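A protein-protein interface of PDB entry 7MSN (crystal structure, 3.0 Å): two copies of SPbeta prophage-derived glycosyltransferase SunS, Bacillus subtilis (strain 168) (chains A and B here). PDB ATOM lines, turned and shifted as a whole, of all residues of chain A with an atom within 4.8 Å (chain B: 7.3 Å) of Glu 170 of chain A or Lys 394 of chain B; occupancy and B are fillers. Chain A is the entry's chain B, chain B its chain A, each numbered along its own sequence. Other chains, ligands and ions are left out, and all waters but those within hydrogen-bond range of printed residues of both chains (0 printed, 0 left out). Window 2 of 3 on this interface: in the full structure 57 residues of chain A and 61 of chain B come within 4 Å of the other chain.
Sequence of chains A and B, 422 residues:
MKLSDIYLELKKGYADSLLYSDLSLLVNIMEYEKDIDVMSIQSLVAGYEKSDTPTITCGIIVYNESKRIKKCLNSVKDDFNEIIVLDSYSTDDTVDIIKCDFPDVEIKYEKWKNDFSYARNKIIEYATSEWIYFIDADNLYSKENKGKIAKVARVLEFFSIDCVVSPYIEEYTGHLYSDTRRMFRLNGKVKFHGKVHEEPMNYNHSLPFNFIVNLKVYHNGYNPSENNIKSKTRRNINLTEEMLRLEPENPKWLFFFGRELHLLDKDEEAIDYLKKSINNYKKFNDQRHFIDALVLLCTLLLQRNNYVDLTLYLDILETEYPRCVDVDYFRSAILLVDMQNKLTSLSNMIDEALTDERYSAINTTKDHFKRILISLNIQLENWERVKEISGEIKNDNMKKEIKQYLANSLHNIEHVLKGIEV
No position is printed for both chains.
Glu 170 of chain A touches just one residue of chain B: Lys 394 (3.5 Å). Of chain A, only Glu 170, Tyr 172 and Gly 174 come within 4 Å of Lys 394 of chain B. Of the printed residues of chain A, Thr 365 of chain B touches Gly 174 (3.5 Å). Of the printed residues of chain B, Tyr 172 of chain A touches Lys 394 (3.8 Å) and Asn 397 (3.97 Å). The nearest residue of chain B that does not touch Glu 170 of chain A is Thr 365 of chain B (6.4 Å). The nearest printed residue of chain A that does not touch Asn 397 of chain B is Thr 173 of chain A (5.8 Å).
Among the printed residues, pairs that only touch across the chains: Tyr 172 of chain A with Lys 394 of chain B, Tyr 172 of chain A with Asn 397 of chain B, Thr 173 of chain A with Asn 395 of chain B, Gly 174 of chain A with Thr 365 of chain B and Gly 174 of chain A with Lys 394 of chain B.
The side-chain amino group (NZ) of Lys 394 of chain B lies within salt-bridge range of the side-chain carboxylate (OE2) of Glu 170 of chain A, 3.5 Å away.
The backbone carbonyl oxygen of Thr 365 of chain B lies within hydrogen-bond range of the side-chain amino group of Lys 370 of chain B (3.2 Å). OD2 of Asp 367 of chain B is in hydrogen-bond range of N of Lys 394 of chain B (3.2 Å). OD2 of Asp 367 of chain B is in hydrogen-bond range of N of Asn 395 of chain B (3.2 Å). The backbone NH of Asn 397 of chain B sits at hydrogen-bond distance from the side-chain amide oxygen of Asn 395 of chain B (3.1 Å). The side-chain amide nitrogen (ND2) of Asn 395 of chain B sits close to the backbone NH (N) of Met 398 of chain B (3.4 Å). The backbone carbonyl oxygen (O) of Glu 170 of chain A lies within hydrogen-bond range of the backbone NH (N) of His 219 of chain A (3.5 Å).
Printed residues of chain A that touch a printed residue of chain B: Glu 170, Tyr 172, Thr 173 and Gly 174. Hydrophobic or aromatic side chains of chain A within 4 Å of the printed part of chain B: Tyr 172. Along chain A the printed residues that touch a printed residue of chain B span positions 170 to 174. Of the 14 printed residues of chain B, 4 touch a printed residue of chain A. Among the printed residues, 6 pairs touch across the chains.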
ATOM      1  N   TYR A 168      35.109 -17.467  20.560  1.00  0.00           N
ATOM      2  CA  TYR A 168      34.713 -18.308  21.683  1.00  0.00           C
ATOM      3  C   TYR A 168      35.162 -19.748  21.452  1.00  0.00           C
ATOM      4  O   TYR A 168      34.787 -20.351  20.444  1.00  0.00           O
ATOM      5  CB  TYR A 168      33.201 -18.276  21.862  1.00  0.00           C
ATOM      6  CG  TYR A 168      32.627 -16.979  22.372  1.00  0.00           C
ATOM      7  CD1 TYR A 168      32.550 -16.721  23.736  1.00  0.00           C
ATOM      8  CD2 TYR A 168      32.114 -16.023  21.497  1.00  0.00           C
ATOM      9  CE1 TYR A 168      32.003 -15.538  24.217  1.00  0.00           C
ATOM     10  CE2 TYR A 168      31.563 -14.833  21.973  1.00  0.00           C
ATOM     11  CZ  TYR A 168      31.511 -14.596  23.336  1.00  0.00           C
ATOM     12  OH  TYR A 168      30.967 -13.422  23.825  1.00  0.00           O
ATOM     13  N   ILE A 169      35.925 -20.322  22.387  1.00  0.00           N
ATOM     14  CA  ILE A 169      36.207 -21.760  22.366  1.00  0.00           C
ATOM     15  C   ILE A 169      35.325 -22.473  23.388  1.00  0.00           C
ATOM     16  O   ILE A 169      35.382 -22.170  24.585  1.00  0.00           O
ATOM     17  CB  ILE A 169      37.682 -22.073  22.640  1.00  0.00           C
ATOM     18  CG1 ILE A 169      38.599 -21.353  21.656  1.00  0.00           C
ATOM     19  CG2 ILE A 169      37.907 -23.592  22.584  1.00  0.00           C
ATOM     20  CD1 ILE A 169      40.025 -21.689  21.878  1.00  0.00           C
ATOM     21  N   GLU A 170      34.542 -23.450  22.926  1.00  0.00           N
ATOM     22  CA  GLU A 170      33.701 -24.270  23.784  1.00  0.00           C
ATOM     23  C   GLU A 170      34.400 -25.585  24.109  1.00  0.00           C
ATOM     24  O   GLU A 170      34.469 -26.475  23.257  1.00  0.00           O
ATOM     25  CB  GLU A 170      32.365 -24.534  23.105  1.00  0.00           C
ATOM     26  CG  GLU A 170      31.409 -25.387  23.922  1.00  0.00           C
ATOM     27  CD  GLU A 170      29.992 -25.353  23.387  1.00  0.00           C
ATOM     28  OE1 GLU A 170      29.219 -24.434  23.766  1.00  0.00           O
ATOM     29  OE2 GLU A 170      29.668 -26.237  22.567  1.00  0.00           O
ATOM     30  N   GLU A 171      34.896 -25.711  25.348  1.00  0.00           N
ATOM     31  CA  GLU A 171      35.339 -26.964  25.960  1.00  0.00           C
ATOM     32  C   GLU A 171      34.371 -28.109  25.683  1.00  0.00           C
ATOM     33  O   GLU A 171      33.168 -27.874  25.496  1.00  0.00           O
ATOM     34  CB  GLU A 171      35.426 -26.809  27.473  1.00  0.00           C
ATOM     35  CG  GLU A 171      36.645 -26.107  27.990  1.00  0.00           C
ATOM     36  CD  GLU A 171      37.825 -27.020  28.061  1.00  0.00           C
ATOM     37  OE1 GLU A 171      37.629 -28.228  27.806  1.00  0.00           O
ATOM     38  OE2 GLU A 171      38.937 -26.534  28.362  1.00  0.00           O
ATOM     39  N   TYR A 172      34.855 -29.358  25.706  1.00  0.00           N
ATOM     40  CA  TYR A 172      33.936 -30.493  25.566  1.00  0.00           C
ATOM     41  C   TYR A 172      32.963 -30.546  26.730  1.00  0.00           C
ATOM     42  O   TYR A 172      31.897 -31.169  26.625  1.00  0.00           O
ATOM     43  CB  TYR A 172      34.710 -31.817  25.479  1.00  0.00           C
ATOM     44  CG  TYR A 172      35.511 -32.112  26.716  1.00  0.00           C
ATOM     45  CD1 TYR A 172      34.952 -32.807  27.789  1.00  0.00           C
ATOM     46  CD2 TYR A 172      36.789 -31.614  26.854  1.00  0.00           C
ATOM     47  CE1 TYR A 172      35.679 -33.042  28.930  1.00  0.00           C
ATOM     48  CE2 TYR A 172      37.508 -31.834  27.987  1.00  0.00           C
ATOM     49  CZ  TYR A 172      36.956 -32.546  29.019  1.00  0.00           C
ATOM     50  OH  TYR A 172      37.710 -32.744  30.143  1.00  0.00           O
ATOM     51  N   THR A 173      33.338 -29.910  27.841  1.00  0.00           N
ATOM     52  CA  THR A 173      32.500 -29.723  29.007  1.00  0.00           C
ATOM     53  C   THR A 173      31.393 -28.722  28.765  1.00  0.00           C
ATOM     54  O   THR A 173      30.497 -28.610  29.598  1.00  0.00           O
ATOM     55  CB  THR A 173      33.363 -29.245  30.163  1.00  0.00           C
ATOM     56  OG1 THR A 173      33.799 -27.919  29.877  1.00  0.00           O
ATOM     57  CG2 THR A 173      34.587 -30.121  30.314  1.00  0.00           C
ATOM     58  N   GLY A 174      31.424 -27.997  27.656  1.00  0.00           N
ATOM     59  CA  GLY A 174      30.513 -26.899  27.453  1.00  0.00           C
ATOM     60  C   GLY A 174      31.014 -25.579  27.984  1.00  0.00           C
ATOM     61  O   GLY A 174      30.439 -24.541  27.638  1.00  0.00           O
ATOM     62  N   HIS A 175      32.059 -25.593  28.820  1.00  0.00           N
ATOM     63  CA  HIS A 175      32.678 -24.360  29.292  1.00  0.00           C
ATOM     64  C   HIS A 175      33.249 -23.607  28.121  1.00  0.00           C
ATOM     65  O   HIS A 175      33.869 -24.183  27.234  1.00  0.00           O
ATOM     66  CB  HIS A 175      33.790 -24.625  30.306  1.00  0.00           C
ATOM     67  CG  HIS A 175      34.475 -23.377  30.794  1.00  0.00           C
ATOM     68  ND1 HIS A 175      33.813 -22.378  31.475  1.00  0.00           N
ATOM     69  CD2 HIS A 175      35.769 -22.987  30.733  1.00  0.00           C
ATOM     70  CE1 HIS A 175      34.664 -21.414  31.781  1.00  0.00           C
ATOM     71  NE2 HIS A 175      35.858 -21.760  31.344  1.00  0.00           N
ATOM     72  N   LEU A 176      33.071 -22.307  28.148  1.00  0.00           N
ATOM     73  CA  LEU A 176      33.205 -21.480  26.968  1.00  0.00           C
ATOM     74  C   LEU A 176      34.256 -20.428  27.302  1.00  0.00           C
ATOM     75  O   LEU A 176      34.036 -19.603  28.190  1.00  0.00           O
ATOM     76  CB  LEU A 176      31.832 -20.905  26.658  1.00  0.00           C
ATOM     77  CG  LEU A 176      31.490 -20.095  25.434  1.00  0.00           C
ATOM     78  CD1 LEU A 176      31.704 -20.955  24.225  1.00  0.00           C
ATOM     79  CD2 LEU A 176      30.052 -19.723  25.546  1.00  0.00           C
ATOM     80  N   VAL A 217      34.451 -22.147  18.092  1.00  0.00           N
ATOM     81  CA  VAL A 217      35.187 -23.362  17.791  1.00  0.00           C
ATOM     82  C   VAL A 217      34.824 -24.352  18.888  1.00  0.00           C
ATOM     83  O   VAL A 217      34.575 -23.969  20.033  1.00  0.00           O
ATOM     84  CB  VAL A 217      36.719 -23.155  17.758  1.00  0.00           C
ATOM     85  CG1 VAL A 217      37.129 -22.053  16.784  1.00  0.00           C
ATOM     86  CG2 VAL A 217      37.275 -22.992  19.109  1.00  0.00           C
ATOM     87  N   TYR A 218      34.794 -25.627  18.536  1.00  0.00           N
ATOM     88  CA  TYR A 218      34.331 -26.682  19.419  1.00  0.00           C
ATOM     89  C   TYR A 218      35.385 -27.771  19.534  1.00  0.00           C
ATOM     90  O   TYR A 218      36.257 -27.910  18.677  1.00  0.00           O
ATOM     91  CB  TYR A 218      33.024 -27.302  18.903  1.00  0.00           C
ATOM     92  CG  TYR A 218      31.863 -26.350  18.697  1.00  0.00           C
ATOM     93  CD1 TYR A 218      31.278 -25.685  19.775  1.00  0.00           C
ATOM     94  CD2 TYR A 218      31.327 -26.138  17.430  1.00  0.00           C
ATOM     95  CE1 TYR A 218      30.197 -24.824  19.593  1.00  0.00           C
ATOM     96  CE2 TYR A 218      30.240 -25.285  17.243  1.00  0.00           C
ATOM     97  CZ  TYR A 218      29.686 -24.632  18.327  1.00  0.00           C
ATOM     98  OH  TYR A 218      28.619 -23.786  18.144  1.00  0.00           O
ATOM     99  N   HIS A 219      35.280 -28.565  20.596  1.00  0.00           N
ATOM    100  CA  HIS A 219      36.104 -29.753  20.725  1.00  0.00           C
ATOM    101  C   HIS A 219      35.775 -30.758  19.618  1.00  0.00           C
ATOM    102  O   HIS A 219      34.810 -30.608  18.861  1.00  0.00           O
ATOM    103  CB  HIS A 219      35.926 -30.373  22.107  1.00  0.00           C
ATOM    104  CG  HIS A 219      36.815 -31.550  22.358  1.00  0.00           C
ATOM    105  ND1 HIS A 219      36.474 -32.832  21.980  1.00  0.00           N
ATOM    106  CD2 HIS A 219      38.056 -31.635  22.892  1.00  0.00           C
ATOM    107  CE1 HIS A 219      37.453 -33.660  22.297  1.00  0.00           C
ATOM    108  NE2 HIS A 219      38.424 -32.960  22.853  1.00  0.00           N
ATOM    109  N   THR B 365      28.661 -23.012  31.895  1.00  0.00           N
ATOM    110  CA  THR B 365      27.370 -23.692  31.877  1.00  0.00           C
ATOM    111  C   THR B 365      26.678 -23.673  33.229  1.00  0.00           C
ATOM    112  O   THR B 365      25.523 -24.121  33.326  1.00  0.00           O
ATOM    113  CB  THR B 365      27.528 -25.135  31.434  1.00  0.00           C
ATOM    114  OG1 THR B 365      28.564 -25.729  32.206  1.00  0.00           O
ATOM    115  CG2 THR B 365      27.907 -25.206  29.987  1.00  0.00           C
ATOM    116  N   ASP B 367      27.020 -25.681  35.276  1.00  0.00           N
ATOM    117  CA  ASP B 367      26.689 -27.077  35.528  1.00  0.00           C
ATOM    118  C   ASP B 367      27.056 -27.529  36.918  1.00  0.00           C
ATOM    119  O   ASP B 367      26.636 -28.615  37.317  1.00  0.00           O
ATOM    120  CB  ASP B 367      27.413 -28.023  34.574  1.00  0.00           C
ATOM    121  CG  ASP B 367      26.708 -28.195  33.262  1.00  0.00           C
ATOM    122  OD1 ASP B 367      25.630 -27.554  33.064  1.00  0.00           O
ATOM    123  OD2 ASP B 367      27.258 -28.981  32.446  1.00  0.00           O
ATOM    124  N   LYS B 370      24.055 -26.716  38.994  1.00  0.00           N
ATOM    125  CA  LYS B 370      22.994 -27.664  38.734  1.00  0.00           C
ATOM    126  C   LYS B 370      23.227 -28.946  39.524  1.00  0.00           C
ATOM    127  O   LYS B 370      22.262 -29.572  39.968  1.00  0.00           O
ATOM    128  CB  LYS B 370      22.890 -27.878  37.219  1.00  0.00           C
ATOM    129  CG  LYS B 370      22.262 -26.659  36.506  1.00  0.00           C
ATOM    130  CD  LYS B 370      22.462 -26.661  35.003  1.00  0.00           C
ATOM    131  CE  LYS B 370      22.212 -25.276  34.394  1.00  0.00           C
ATOM    132  NZ  LYS B 370      22.565 -25.218  32.948  1.00  0.00           N
ATOM    133  N   ILE B 389      16.198 -30.894  35.852  1.00  0.00           N
ATOM    134  CA  ILE B 389      17.512 -30.283  35.961  1.00  0.00           C
ATOM    135  C   ILE B 389      18.589 -31.156  35.322  1.00  0.00           C
ATOM    136  O   ILE B 389      19.508 -30.646  34.672  1.00  0.00           O
ATOM    137  CB  ILE B 389      17.791 -30.017  37.445  1.00  0.00           C
ATOM    138  CG1 ILE B 389      17.114 -28.720  37.888  1.00  0.00           C
ATOM    139  CG2 ILE B 389      19.264 -29.983  37.699  1.00  0.00           C
ATOM    140  CD1 ILE B 389      17.230 -28.483  39.389  1.00  0.00           C
ATOM    141  N   SER B 390      18.506 -32.479  35.490  1.00  0.00           N
ATOM    142  CA  SER B 390      19.545 -33.346  34.923  1.00  0.00           C
ATOM    143  C   SER B 390      19.439 -33.493  33.409  1.00  0.00           C
ATOM    144  O   SER B 390      20.265 -34.193  32.814  1.00  0.00           O
ATOM    145  CB  SER B 390      19.508 -34.736  35.560  1.00  0.00           C
ATOM    146  OG  SER B 390      18.455 -35.490  34.994  1.00  0.00           O
ATOM    147  N   GLY B 391      18.446 -32.874  32.775  1.00  0.00           N
ATOM    148  CA  GLY B 391      18.363 -32.902  31.333  1.00  0.00           C
ATOM    149  C   GLY B 391      19.154 -31.767  30.738  1.00  0.00           C
ATOM    150  O   GLY B 391      19.643 -31.857  29.612  1.00  0.00           O
ATOM    151  N   GLU B 392      19.312 -30.699  31.517  1.00  0.00           N
ATOM    152  CA  GLU B 392      19.936 -29.467  31.059  1.00  0.00           C
ATOM    153  C   GLU B 392      21.422 -29.375  31.408  1.00  0.00           C
ATOM    154  O   GLU B 392      21.973 -28.268  31.396  1.00  0.00           O
ATOM    155  CB  GLU B 392      19.207 -28.257  31.648  1.00  0.00           C
ATOM    156  CG  GLU B 392      17.744 -28.156  31.292  1.00  0.00           C
ATOM    157  CD  GLU B 392      16.952 -27.437  32.369  1.00  0.00           C
ATOM    158  OE1 GLU B 392      15.846 -26.935  32.066  1.00  0.00           O
ATOM    159  OE2 GLU B 392      17.446 -27.355  33.515  1.00  0.00           O
ATOM    160  N   ILE B 393      22.086 -30.491  31.744  1.00  0.00           N
ATOM    161  CA  ILE B 393      23.530 -30.436  31.957  1.00  0.00           C
ATOM    162  C   ILE B 393      24.201 -30.947  30.691  1.00  0.00           C
ATOM    163  O   ILE B 393      23.751 -31.938  30.090  1.00  0.00           O
ATOM    164  CB  ILE B 393      24.031 -31.237  33.176  1.00  0.00           C
ATOM    165  CG1 ILE B 393      23.879 -32.727  32.971  1.00  0.00           C
ATOM    166  CG2 ILE B 393      23.258 -30.854  34.432  1.00  0.00           C
ATOM    167  CD1 ILE B 393      24.630 -33.470  34.009  1.00  0.00           C
ATOM    168  N   LYS B 394      25.295 -30.276  30.288  1.00  0.00           N
ATOM    169  CA  LYS B 394      25.915 -30.521  28.996  1.00  0.00           C
ATOM    170  C   LYS B 394      27.250 -31.262  29.124  1.00  0.00           C
ATOM    171  O   LYS B 394      27.729 -31.830  28.137  1.00  0.00           O
ATOM    172  CB  LYS B 394      26.075 -29.176  28.245  1.00  0.00           C
ATOM    173  CG  LYS B 394      26.387 -29.284  26.735  1.00  0.00           C
ATOM    174  CD  LYS B 394      27.863 -29.321  26.328  1.00  0.00           C
ATOM    175  CE  LYS B 394      28.007 -29.203  24.799  1.00  0.00           C
ATOM    176  NZ  LYS B 394      29.437 -29.254  24.377  1.00  0.00           N
ATOM    177  N   ASN B 395      27.832 -31.326  30.323  1.00  0.00           N
ATOM    178  CA  ASN B 395      29.057 -32.092  30.549  1.00  0.00           C
ATOM    179  C   ASN B 395      28.694 -33.560  30.720  1.00  0.00           C
ATOM    180  O   ASN B 395      28.103 -33.953  31.736  1.00  0.00           O
ATOM    181  CB  ASN B 395      29.823 -31.574  31.767  1.00  0.00           C
ATOM    182  CG  ASN B 395      30.949 -32.534  32.226  1.00  0.00           C
ATOM    183  OD1 ASN B 395      31.570 -33.235  31.411  1.00  0.00           O
ATOM    184  ND2 ASN B 395      31.226 -32.538  33.533  1.00  0.00           N
ATOM    185  N   ASP B 396      29.080 -34.371  29.733  1.00  0.00           N
ATOM    186  CA  ASP B 396      28.724 -35.783  29.719  1.00  0.00           C
ATOM    187  C   ASP B 396      29.279 -36.528  30.926  1.00  0.00           C
ATOM    188  O   ASP B 396      28.723 -37.556  31.320  1.00  0.00           O
ATOM    189  CB  ASP B 396      29.224 -36.425  28.426  1.00  0.00           C
ATOM    190  CG  ASP B 396      28.420 -35.998  27.211  1.00  0.00           C
ATOM    191  OD1 ASP B 396      27.591 -35.068  27.339  1.00  0.00           O
ATOM    192  OD2 ASP B 396      28.641 -36.572  26.119  1.00  0.00           O
ATOM    193  N   ASN B 397      30.372 -36.053  31.520  1.00  0.00           N
ATOM    194  CA  ASN B 397      30.948 -36.795  32.641  1.00  0.00           C
ATOM    195  C   ASN B 397      30.146 -36.622  33.921  1.00  0.00           C
ATOM    196  O   ASN B 397      30.101 -37.536  34.751  1.00  0.00           O
ATOM    197  CB  ASN B 397      32.401 -36.383  32.865  1.00  0.00           C
ATOM    198  CG  ASN B 397      33.286 -36.743  31.696  1.00  0.00           C
ATOM    199  OD1 ASN B 397      33.808 -35.861  31.002  1.00  0.00           O
ATOM    200  ND2 ASN B 397      33.485 -38.051  31.486  1.00  0.00           N
ATOM    201  N   MET B 398      29.521 -35.464  34.105  1.00  0.00           N
ATOM    202  CA  MET B 398      28.629 -35.285  35.241  1.00  0.00           C
ATOM    203  C   MET B 398      27.357 -36.097  35.052  1.00  0.00           C
ATOM    204  O   MET B 398      26.906 -36.797  35.964  1.00  0.00           O
ATOM    205  CB  MET B 398      28.320 -33.805  35.394  1.00  0.00           C
ATOM    206  CG  MET B 398      27.473 -33.466  36.555  1.00  0.00           C
ATOM    207  SD  MET B 398      27.263 -31.711  36.498  1.00  0.00           S
ATOM    208  CE  MET B 398      28.790 -31.278  37.324  1.00  0.00           C
ATOM    209  N   LYS B 399      26.783 -36.024  33.855  1.00  0.00           N
ATOM    210  CA  LYS B 399      25.609 -36.813  33.517  1.00  0.00           C
ATOM    211  C   LYS B 399      25.883 -38.308  33.693  1.00  0.00           C
ATOM    212  O   LYS B 399      24.969 -39.067  34.035  1.00  0.00           O
ATOM    213  CB  LYS B 399      25.200 -36.419  32.096  1.00  0.00           C
ATOM    214  CG  LYS B 399      23.932 -36.949  31.559  1.00  0.00           C
ATOM    215  CD  LYS B 399      23.756 -36.456  30.124  1.00  0.00           C
ATOM    216  CE  LYS B 399      23.377 -34.981  30.101  1.00  0.00           C
ATOM    217  NZ  LYS B 399      23.041 -34.465  28.739  1.00  0.00           N
